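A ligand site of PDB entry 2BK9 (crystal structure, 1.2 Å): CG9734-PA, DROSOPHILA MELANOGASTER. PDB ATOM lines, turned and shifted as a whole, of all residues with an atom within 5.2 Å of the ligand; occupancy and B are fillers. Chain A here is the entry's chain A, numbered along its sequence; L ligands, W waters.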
ATOM      1  N   PHE A  31      13.795 -17.194  12.691  1.00  0.00           N
ATOM      2  CA  PHE A  31      13.955 -16.238  13.782  1.00  0.00           C
ATOM      3  C   PHE A  31      15.362 -15.643  13.780  1.00  0.00           C
ATOM      4  O   PHE A  31      15.532 -14.438  13.839  1.00  0.00           O
ATOM      5  CB  PHE A  31      13.621 -16.970  15.050  1.00  0.00           C
ATOM      6  CG  PHE A  31      13.717 -16.176  16.326  1.00  0.00           C
ATOM      7  CD1 PHE A  31      12.980 -15.018  16.541  1.00  0.00           C
ATOM      8  CD2 PHE A  31      14.481 -16.663  17.353  1.00  0.00           C
ATOM      9  CE1 PHE A  31      13.014 -14.363  17.742  1.00  0.00           C
ATOM     10  CE2 PHE A  31      14.490 -16.024  18.576  1.00  0.00           C
ATOM     11  CZ  PHE A  31      13.751 -14.865  18.761  1.00  0.00           C
ATOM     12  N   ASN A  38      19.098 -12.274  18.553  1.00  0.00           N
ATOM     13  CA  ASN A  38      18.606 -13.294  19.450  1.00  0.00           C
ATOM     14  C   ASN A  38      19.574 -14.482  19.590  1.00  0.00           C
ATOM     15  O   ASN A  38      19.546 -15.150  20.604  1.00  0.00           O
ATOM     16  CB  ASN A  38      17.261 -13.796  18.977  1.00  0.00           C
ATOM     17  CG  ASN A  38      16.192 -12.724  19.065  1.00  0.00           C
ATOM     18  OD1 ASN A  38      15.778 -12.367  20.168  1.00  0.00           O
ATOM     19  ND2 ASN A  38      15.784 -12.183  17.912  1.00  0.00           N
ATOM     20  N   LYS A  41      21.736 -14.887  22.861  1.00  0.00           N
ATOM     21  CA  LYS A  41      21.195 -15.392  24.103  1.00  0.00           C
ATOM     22  C   LYS A  41      21.543 -16.861  24.338  1.00  0.00           C
ATOM     23  O   LYS A  41      21.404 -17.353  25.431  1.00  0.00           O
ATOM     24  CB  LYS A  41      19.679 -15.259  24.104  1.00  0.00           C
ATOM     25  CG  LYS A  41      19.153 -13.868  24.012  1.00  0.00           C
ATOM     26  CD  LYS A  41      19.384 -13.037  25.199  1.00  0.00           C
ATOM     27  CE  LYS A  41      18.656 -11.724  25.213  1.00  0.00           C
ATOM     28  NZ  LYS A  41      18.935 -10.948  26.456  1.00  0.00           N
ATOM     29  N   PHE A  42      21.951 -17.573  23.275  1.00  0.00           N
ATOM     30  CA  PHE A  42      22.128 -19.031  23.322  1.00  0.00           C
ATOM     31  C   PHE A  42      23.601 -19.409  23.284  1.00  0.00           C
ATOM     32  O   PHE A  42      24.415 -18.734  22.684  1.00  0.00           O
ATOM     33  CB  PHE A  42      21.446 -19.676  22.128  1.00  0.00           C
ATOM     34  CG  PHE A  42      19.962 -19.667  22.186  1.00  0.00           C
ATOM     35  CD1 PHE A  42      19.302 -20.662  22.895  1.00  0.00           C
ATOM     36  CD2 PHE A  42      19.219 -18.660  21.549  1.00  0.00           C
ATOM     37  CE1 PHE A  42      17.941 -20.729  22.914  1.00  0.00           C
ATOM     38  CE2 PHE A  42      17.808 -18.757  21.591  1.00  0.00           C
ATOM     39  CZ  PHE A  42      17.211 -19.806  22.246  1.00  0.00           C
ATOM     40  N   PRO A  43      23.930 -20.598  23.781  1.00  0.00           N
ATOM     41  CA  PRO A  43      25.324 -21.058  23.739  1.00  0.00           C
ATOM     42  C   PRO A  43      25.873 -21.323  22.356  1.00  0.00           C
ATOM     43  O   PRO A  43      27.072 -21.285  22.128  1.00  0.00           O
ATOM     44  CB  PRO A  43      25.288 -22.340  24.564  1.00  0.00           C
ATOM     45  CG  PRO A  43      23.855 -22.721  24.688  1.00  0.00           C
ATOM     46  CD  PRO A  43      23.075 -21.492  24.575  1.00  0.00           C
ATOM     47  N   ARG A  57      21.718 -28.206  21.081  1.00  0.00           N
ATOM     48  CA  ARG A  57      20.967 -27.267  21.868  1.00  0.00           C
ATOM     49  C   ARG A  57      19.979 -26.480  21.038  1.00  0.00           C
ATOM     50  O   ARG A  57      18.895 -26.156  21.499  1.00  0.00           O
ATOM     51  CB  ARG A  57      21.922 -26.407  22.671  1.00  0.00           C
ATOM     52  CG  ARG A  57      22.554 -27.187  23.808  1.00  0.00           C
ATOM     53  CD  ARG A  57      23.468 -26.365  24.674  1.00  0.00           C
ATOM     54  NE  ARG A  57      23.821 -27.117  25.892  1.00  0.00           N
ATOM     55  CZ  ARG A  57      24.628 -28.165  25.952  1.00  0.00           C
ATOM     56  NH1 ARG A  57      25.261 -28.591  24.883  1.00  0.00           N
ATOM     57  NH2 ARG A  57      24.838 -28.802  27.120  1.00  0.00           N
ATOM     58  N   HIS A  61      15.816 -26.509  21.703  1.00  0.00           N
ATOM     59  CA  HIS A  61      14.896 -25.373  21.801  1.00  0.00           C
ATOM     60  C   HIS A  61      13.835 -25.410  20.715  1.00  0.00           C
ATOM     61  O   HIS A  61      12.682 -25.094  20.950  1.00  0.00           O
ATOM     62  CB  HIS A  61      15.666 -24.028  21.785  1.00  0.00           C
ATOM     63  CG  HIS A  61      14.824 -22.883  22.218  1.00  0.00           C
ATOM     64  ND1 HIS A  61      14.087 -22.108  21.360  1.00  0.00           N
ATOM     65  CD2 HIS A  61      14.562 -22.394  23.451  1.00  0.00           C
ATOM     66  CE1 HIS A  61      13.409 -21.203  22.061  1.00  0.00           C
ATOM     67  NE2 HIS A  61      13.692 -21.346  23.334  1.00  0.00           N
ATOM     68  N   ARG A  64      11.274 -27.788  21.793  1.00  0.00           N
ATOM     69  CA  ARG A  64      10.478 -27.227  22.864  1.00  0.00           C
ATOM     70  C   ARG A  64       9.375 -26.369  22.323  1.00  0.00           C
ATOM     71  O   ARG A  64       8.264 -26.402  22.835  1.00  0.00           O
ATOM     72  CB  ARG A  64      11.345 -26.414  23.824  1.00  0.00           C
ATOM     73  CG  ARG A  64      12.120 -27.290  24.850  1.00  0.00           C
ATOM     74  CD  ARG A  64      13.199 -26.577  25.644  1.00  0.00           C
ATOM     75  NE  ARG A  64      13.650 -27.429  26.753  1.00  0.00           N
ATOM     76  CZ  ARG A  64      14.880 -27.836  26.984  1.00  0.00           C
ATOM     77  NH1 ARG A  64      15.899 -27.418  26.279  1.00  0.00           N
ATOM     78  NH2 ARG A  64      15.083 -28.634  28.012  1.00  0.00           N
ATOM     79  N   ILE A  65       9.663 -25.525  21.350  1.00  0.00           N
ATOM     80  CA  ILE A  65       8.606 -24.664  20.816  1.00  0.00           C
ATOM     81  C   ILE A  65       7.479 -25.557  20.276  1.00  0.00           C
ATOM     82  O   ILE A  65       6.309 -25.310  20.522  1.00  0.00           O
ATOM     83  CB  ILE A  65       9.196 -23.752  19.730  1.00  0.00           C
ATOM     84  CG1 ILE A  65      10.138 -22.716  20.344  1.00  0.00           C
ATOM     85  CG2 ILE A  65       8.068 -23.074  18.971  1.00  0.00           C
ATOM     86  CD1 ILE A  65      10.928 -21.934  19.354  1.00  0.00           C
ATOM     87  N   VAL A  68       5.572 -27.395  23.242  1.00  0.00           N
ATOM     88  CA  VAL A  68       4.743 -26.539  24.044  1.00  0.00           C
ATOM     89  C   VAL A  68       3.482 -26.126  23.284  1.00  0.00           C
ATOM     90  O   VAL A  68       2.405 -26.072  23.864  1.00  0.00           O
ATOM     91  CB  VAL A  68       5.558 -25.305  24.547  1.00  0.00           C
ATOM     92  CG1 VAL A  68       4.690 -24.280  25.232  1.00  0.00           C
ATOM     93  CG2 VAL A  68       6.655 -25.789  25.520  1.00  0.00           C
ATOM     94  N   PHE A  69       3.613 -25.817  22.002  1.00  0.00           N
ATOM     95  CA  PHE A  69       2.407 -25.616  21.207  1.00  0.00           C
ATOM     96  C   PHE A  69       1.540 -26.865  21.160  1.00  0.00           C
ATOM     97  O   PHE A  69       0.335 -26.772  21.267  1.00  0.00           O
ATOM     98  CB  PHE A  69       2.766 -25.119  19.808  1.00  0.00           C
ATOM     99  CG  PHE A  69       2.839 -23.629  19.753  1.00  0.00           C
ATOM    100  CD1 PHE A  69       4.011 -22.958  19.878  1.00  0.00           C
ATOM    101  CD2 PHE A  69       1.674 -22.855  19.748  1.00  0.00           C
ATOM    102  CE1 PHE A  69       4.026 -21.562  19.868  1.00  0.00           C
ATOM    103  CE2 PHE A  69       1.720 -21.511  19.745  1.00  0.00           C
ATOM    104  CZ  PHE A  69       2.915 -20.869  19.779  1.00  0.00           C
ATOM    105  N   TRP A  89       1.816 -21.137  29.775  1.00  0.00           N
ATOM    106  CA  TRP A  89       2.499 -19.970  29.194  1.00  0.00           C
ATOM    107  C   TRP A  89       3.050 -19.025  30.258  1.00  0.00           C
ATOM    108  O   TRP A  89       4.003 -18.328  29.998  1.00  0.00           O
ATOM    109  CB  TRP A  89       1.605 -19.305  28.167  1.00  0.00           C
ATOM    110  CG  TRP A  89       1.494 -20.180  26.961  1.00  0.00           C
ATOM    111  CD1 TRP A  89       0.503 -21.096  26.672  1.00  0.00           C
ATOM    112  CD2 TRP A  89       2.443 -20.291  25.930  1.00  0.00           C
ATOM    113  NE1 TRP A  89       0.810 -21.748  25.517  1.00  0.00           N
ATOM    114  CE2 TRP A  89       1.993 -21.266  25.040  1.00  0.00           C
ATOM    115  CE3 TRP A  89       3.638 -19.648  25.652  1.00  0.00           C
ATOM    116  CZ2 TRP A  89       2.683 -21.584  23.876  1.00  0.00           C
ATOM    117  CZ3 TRP A  89       4.321 -19.971  24.509  1.00  0.00           C
ATOM    118  CH2 TRP A  89       3.834 -20.922  23.622  1.00  0.00           C
ATOM    119  N   ILE A  92       6.373 -20.666  30.787  1.00  0.00           N
ATOM    120  CA  ILE A  92       7.297 -20.290  29.727  1.00  0.00           C
ATOM    121  C   ILE A  92       7.817 -18.871  29.940  1.00  0.00           C
ATOM    122  O   ILE A  92       9.013 -18.597  29.853  1.00  0.00           O
ATOM    123  CB  ILE A  92       6.617 -20.392  28.363  1.00  0.00           C
ATOM    124  CG1 ILE A  92       6.254 -21.852  28.037  1.00  0.00           C
ATOM    125  CG2 ILE A  92       7.478 -19.818  27.267  1.00  0.00           C
ATOM    126  CD1 ILE A  92       7.397 -22.802  28.054  1.00  0.00           C
ATOM    127  N   SER A  95      10.273 -18.708  32.769  1.00  0.00           N
ATOM    128  CA  SER A  95      11.511 -19.411  32.428  1.00  0.00           C
ATOM    129  C   SER A  95      12.480 -18.554  31.626  1.00  0.00           C
ATOM    130  O   SER A  95      13.680 -18.840  31.628  1.00  0.00           O
ATOM    131  CB  SER A  95      11.188 -20.687  31.609  1.00  0.00           C
ATOM    132  OG  SER A  95      10.677 -21.681  32.457  1.00  0.00           O
ATOM    133  N   HIS A  96      12.024 -17.548  30.907  1.00  0.00           N
ATOM    134  CA  HIS A  96      12.901 -16.710  30.112  1.00  0.00           C
ATOM    135  C   HIS A  96      13.366 -15.451  30.821  1.00  0.00           C
ATOM    136  O   HIS A  96      14.229 -14.773  30.297  1.00  0.00           O
ATOM    137  CB  HIS A  96      12.235 -16.384  28.777  1.00  0.00           C
ATOM    138  CG  HIS A  96      12.078 -17.557  27.875  1.00  0.00           C
ATOM    139  ND1 HIS A  96      11.033 -18.452  27.971  1.00  0.00           N
ATOM    140  CD2 HIS A  96      12.894 -18.041  26.913  1.00  0.00           C
ATOM    141  CE1 HIS A  96      11.199 -19.407  27.046  1.00  0.00           C
ATOM    142  NE2 HIS A  96      12.315 -19.167  26.373  1.00  0.00           N
ATOM    143  N   ARG A  99      16.968 -14.719  30.969  1.00  0.00           N
ATOM    144  CA  ARG A  99      17.586 -14.481  29.701  1.00  0.00           C
ATOM    145  C   ARG A  99      17.135 -13.161  29.073  1.00  0.00           C
ATOM    146  O   ARG A  99      17.467 -12.879  27.946  1.00  0.00           O
ATOM    147  CB  ARG A  99      17.292 -15.628  28.739  1.00  0.00           C
ATOM    148  CG  ARG A  99      17.887 -16.922  29.147  1.00  0.00           C
ATOM    149  CD  ARG A  99      19.429 -16.873  29.064  1.00  0.00           C
ATOM    150  NE  ARG A  99      19.965 -18.189  29.436  1.00  0.00           N
ATOM    151  CZ  ARG A  99      20.002 -18.687  30.666  1.00  0.00           C
ATOM    152  NH1 ARG A  99      19.729 -17.929  31.719  1.00  0.00           N
ATOM    153  NH2 ARG A  99      20.359 -19.940  30.870  1.00  0.00           N
ATOM    154  N   VAL A 101      14.470 -12.007  27.634  1.00  0.00           N
ATOM    155  CA  VAL A 101      13.789 -12.100  26.350  1.00  0.00           C
ATOM    156  C   VAL A 101      12.703 -11.033  26.309  1.00  0.00           C
ATOM    157  O   VAL A 101      11.725 -11.102  27.072  1.00  0.00           O
ATOM    158  CB  VAL A 101      13.242 -13.499  26.088  1.00  0.00           C
ATOM    159  CG1 VAL A 101      12.472 -13.540  24.801  1.00  0.00           C
ATOM    160  CG2 VAL A 101      14.371 -14.504  26.105  1.00  0.00           C
ATOM    161  N   SER A 105      11.461  -9.347  21.197  1.00  0.00           N
ATOM    162  CA  SER A 105      11.949 -10.658  20.799  1.00  0.00           C
ATOM    163  C   SER A 105      10.823 -11.661  20.660  1.00  0.00           C
ATOM    164  O   SER A 105      10.754 -12.405  19.682  1.00  0.00           O
ATOM    165  CB  SER A 105      12.968 -11.121  21.838  1.00  0.00           C
ATOM    166  OG  SER A 105      13.488 -12.372  21.569  1.00  0.00           O
ATOM    167  N   TYR A 106       9.916 -11.744  21.639  1.00  0.00           N
ATOM    168  CA  TYR A 106       8.751 -12.584  21.503  1.00  0.00           C
ATOM    169  C   TYR A 106       7.944 -12.229  20.238  1.00  0.00           C
ATOM    170  O   TYR A 106       7.497 -13.128  19.519  1.00  0.00           O
ATOM    171  CB  TYR A 106       7.845 -12.525  22.702  1.00  0.00           C
ATOM    172  CG  TYR A 106       8.295 -13.368  23.872  1.00  0.00           C
ATOM    173  CD1 TYR A 106       8.230 -14.745  23.836  1.00  0.00           C
ATOM    174  CD2 TYR A 106       8.731 -12.764  25.044  1.00  0.00           C
ATOM    175  CE1 TYR A 106       8.570 -15.533  24.904  1.00  0.00           C
ATOM    176  CE2 TYR A 106       9.075 -13.538  26.131  1.00  0.00           C
ATOM    177  CZ  TYR A 106       8.969 -14.927  26.078  1.00  0.00           C
ATOM    178  OH  TYR A 106       9.268 -15.705  27.149  1.00  0.00           O
ATOM    179  N   LEU A 109       9.498 -13.615  17.177  1.00  0.00           N
ATOM    180  CA  LEU A 109       9.226 -15.029  17.035  1.00  0.00           C
ATOM    181  C   LEU A 109       7.787 -15.273  16.599  1.00  0.00           C
ATOM    182  O   LEU A 109       7.527 -16.199  15.825  1.00  0.00           O
ATOM    183  CB  LEU A 109       9.530 -15.767  18.346  1.00  0.00           C
ATOM    184  CG  LEU A 109       9.431 -17.290  18.243  1.00  0.00           C
ATOM    185  CD1 LEU A 109      10.455 -17.898  17.345  1.00  0.00           C
ATOM    186  CD2 LEU A 109       9.521 -17.937  19.609  1.00  0.00           C
ATOM    187  N   ILE A 113       6.598 -17.812  13.686  1.00  0.00           N
ATOM    188  CA  ILE A 113       5.760 -18.997  13.917  1.00  0.00           C
ATOM    189  C   ILE A 113       4.572 -19.000  12.981  1.00  0.00           C
ATOM    190  O   ILE A 113       4.275 -19.987  12.321  1.00  0.00           O
ATOM    191  CB  ILE A 113       5.280 -19.033  15.386  1.00  0.00           C
ATOM    192  CG1 ILE A 113       6.470 -19.308  16.312  1.00  0.00           C
ATOM    193  CG2 ILE A 113       4.196 -20.085  15.575  1.00  0.00           C
ATOM    194  CD1 ILE A 113       6.117 -19.070  17.761  1.00  0.00           C
ATOM    195  N   TYR A 139       0.217 -15.168  23.889  1.00  0.00           N
ATOM    196  CA  TYR A 139       1.100 -13.986  24.086  1.00  0.00           C
ATOM    197  C   TYR A 139       0.555 -13.064  25.158  1.00  0.00           C
ATOM    198  O   TYR A 139       1.349 -12.449  25.893  1.00  0.00           O
ATOM    199  CB  TYR A 139       1.327 -13.257  22.776  1.00  0.00           C
ATOM    200  CG  TYR A 139       2.536 -13.763  22.066  1.00  0.00           C
ATOM    201  CD1 TYR A 139       2.776 -15.125  21.847  1.00  0.00           C
ATOM    202  CD2 TYR A 139       3.505 -12.898  21.625  1.00  0.00           C
ATOM    203  CE1 TYR A 139       3.904 -15.601  21.223  1.00  0.00           C
ATOM    204  CE2 TYR A 139       4.679 -13.394  20.997  1.00  0.00           C
ATOM    205  CZ  TYR A 139       4.869 -14.742  20.852  1.00  0.00           C
ATOM    206  OH  TYR A 139       5.988 -15.260  20.249  1.00  0.00           O
HETATM  207  C1  LIG L   1      14.942 -21.871  27.043  1.00  0.00           C
HETATM  208  C2  LIG L   1      10.490 -22.540  25.362  1.00  0.00           C
HETATM  209  C3  LIG L   1      10.871 -18.412  23.010  1.00  0.00           C
HETATM  210  C4  LIG L   1      15.437 -17.983  24.291  1.00  0.00           C
HETATM  211  C5  LIG L   1      13.686 -22.354  26.833  1.00  0.00           C
HETATM  212  C6  LIG L   1      13.078 -23.472  27.569  1.00  0.00           C
HETATM  213  C7  LIG L   1      11.819 -23.667  27.129  1.00  0.00           C
HETATM  214  C8  LIG L   1      11.630 -22.697  26.091  1.00  0.00           C
HETATM  215  C9  LIG L   1      10.738 -24.679  27.539  1.00  0.00           C
HETATM  216  C10 LIG L   1      13.815 -24.257  28.668  1.00  0.00           C
HETATM  217  C11 LIG L   1      13.841 -23.460  29.970  1.00  0.00           C
HETATM  218  C12 LIG L   1      14.681 -24.237  30.941  1.00  0.00           C
HETATM  219  O1  LIG L   1      15.947 -24.177  30.859  1.00  0.00           O
HETATM  220  O2  LIG L   1      14.103 -24.922  31.805  1.00  0.00           O
HETATM  221  C13 LIG L   1      10.211 -21.494  24.520  1.00  0.00           C
HETATM  222  C14 LIG L   1       8.922 -21.268  23.923  1.00  0.00           C
HETATM  223  C15 LIG L   1       9.037 -20.099  23.253  1.00  0.00           C
HETATM  224  C16 LIG L   1      10.344 -19.562  23.479  1.00  0.00           C
HETATM  225  C17 LIG L   1       7.746 -22.196  24.038  1.00  0.00           C
HETATM  226  C18 LIG L   1       7.979 -19.358  22.519  1.00  0.00           C
HETATM  227  C19 LIG L   1       6.982 -19.899  21.849  1.00  0.00           C
HETATM  228  C20 LIG L   1      12.124 -17.915  23.139  1.00  0.00           C
HETATM  229  C21 LIG L   1      12.634 -16.667  22.601  1.00  0.00           C
HETATM  230  C22 LIG L   1      13.924 -16.563  22.898  1.00  0.00           C
HETATM  231  C23 LIG L   1      14.258 -17.727  23.676  1.00  0.00           C
HETATM  232  C24 LIG L   1      11.773 -15.656  21.833  1.00  0.00           C
HETATM  233  C25 LIG L   1      14.825 -15.426  22.492  1.00  0.00           C
HETATM  234  C26 LIG L   1      16.126 -15.457  22.287  1.00  0.00           C
HETATM  235  C27 LIG L   1      15.733 -18.997  25.142  1.00  0.00           C
HETATM  236  C28 LIG L   1      16.937 -19.149  25.836  1.00  0.00           C
HETATM  237  C29 LIG L   1      16.813 -20.306  26.636  1.00  0.00           C
HETATM  238  C30 LIG L   1      15.483 -20.786  26.392  1.00  0.00           C
HETATM  239  C31 LIG L   1      18.178 -18.274  25.686  1.00  0.00           C
HETATM  240  C32 LIG L   1      17.867 -20.861  27.562  1.00  0.00           C
HETATM  241  C33 LIG L   1      18.855 -21.719  26.838  1.00  0.00           C
HETATM  242  C34 LIG L   1      19.936 -22.267  27.711  1.00  0.00           C
HETATM  243  O3  LIG L   1      20.900 -22.868  27.179  1.00  0.00           O
HETATM  244  O4  LIG L   1      19.844 -22.120  28.951  1.00  0.00           O
HETATM  245  N1  LIG L   1      12.760 -21.889  25.959  1.00  0.00           N
HETATM  246  N2  LIG L   1      11.086 -20.435  24.237  1.00  0.00           N
HETATM  247  N3  LIG L   1      13.147 -18.547  23.806  1.00  0.00           N
HETATM  248  N4  LIG L   1      14.849 -19.994  25.496  1.00  0.00           N
HETATM  249 FE1  LIG L   1      12.979 -20.243  24.871  1.00  0.00          FE
HETATM  250  O   HOH W   1      21.331 -19.388  27.260  1.00  0.00           O
HETATM  251  O   HOH W   2      21.640 -25.708  27.605  1.00  0.00           O
HETATM  252  O   HOH W   3      17.928 -22.289  30.926  1.00  0.00           O
HETATM  253  O   HOH W   4      17.398 -24.612  28.096  1.00  0.00           O
HETATM  254  O   HOH W   5      23.262 -21.429  28.311  1.00  0.00           O
HETATM  255  O   HOH W   6      20.817 -23.680  24.638  1.00  0.00           O
HETATM  256  O   HOH W   7      12.938 -22.724  33.585  1.00  0.00           O
HETATM  257  O   HOH W   8      15.398 -19.459  29.257  1.00  0.00           O
HETATM  258  O   HOH W   9      11.602 -25.903  31.576  1.00  0.00           O
HETATM  259  O   HOH W  10      21.885 -23.022  30.787  1.00  0.00           O
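NE2 of His 96 is bound to FE1 of the ligand (2.0 Å). NE2 of His 61 is bound to FE1 of the ligand (2.0 Å). The guanidinium group (NH2) of Arg 99 lies within salt-bridge range of an oxygen (O4) of the ligand (2.9 Å).
O of Ile 92 is in hydrogen-bond range of ND1 of His 96, at 2.8 Å. A ring nitrogen (ND1) of His 96 lies within hydrogen-bond range of the side-chain hydroxyl (OH) of Tyr 106 (3.4 Å). The backbone carbonyl oxygen (O) of Arg 99 sits at hydrogen-bond distance from the side-chain amino group (NZ) of Lys 41 (2.8 Å). The side-chain hydroxyl (OG) of Ser 105 sits at hydrogen-bond distance from the side-chain amide oxygen (OD1) of Asn 38, 2.7 Å away.
Residues that only touch the ligand: Phe 31, Asn 38, Lys 41, Phe 42, Pro 43, Arg 64, Val 68, Phe 69, Trp 89, Ile 92, Val 101, Ser 105 and Leu 109. Hydrophobic or aromatic side chains that line the ligand: Phe 31, Phe 42, Pro 43, His 61, Val 68, Phe 69, Trp 89, Ile 92, His 96, Val 101 and Leu 109. Of the 22 residues printed, 16 come within 4 Å of the ligand. The nearest printed residue that does not touch the ligand is Ile 65 (4.05 Å).
Water W3 bridges an oxygen (O1) of the ligand and the guanidinium group of Arg 99. Water W10 lies within hydrogen-bond range of O4 of the ligand (2.9 Å) and NH2 of Arg 99 (3.4 Å). Water W2 lies within hydrogen-bond range of an oxygen (O3) of the ligand (3.0 Å) and the guanidinium group of Arg 57 (3.1 Å). Water W7 lies within hydrogen-bond range of OG of Ser 95 (2.7 Å) and O2 of the ligand (3.1 Å). Water W1 lies within hydrogen-bond range of the backbone carbonyl oxygen (O) of Lys 41 (2.7 Å) and the guanidinium group (NE) of Arg 99 (2.8 Å).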
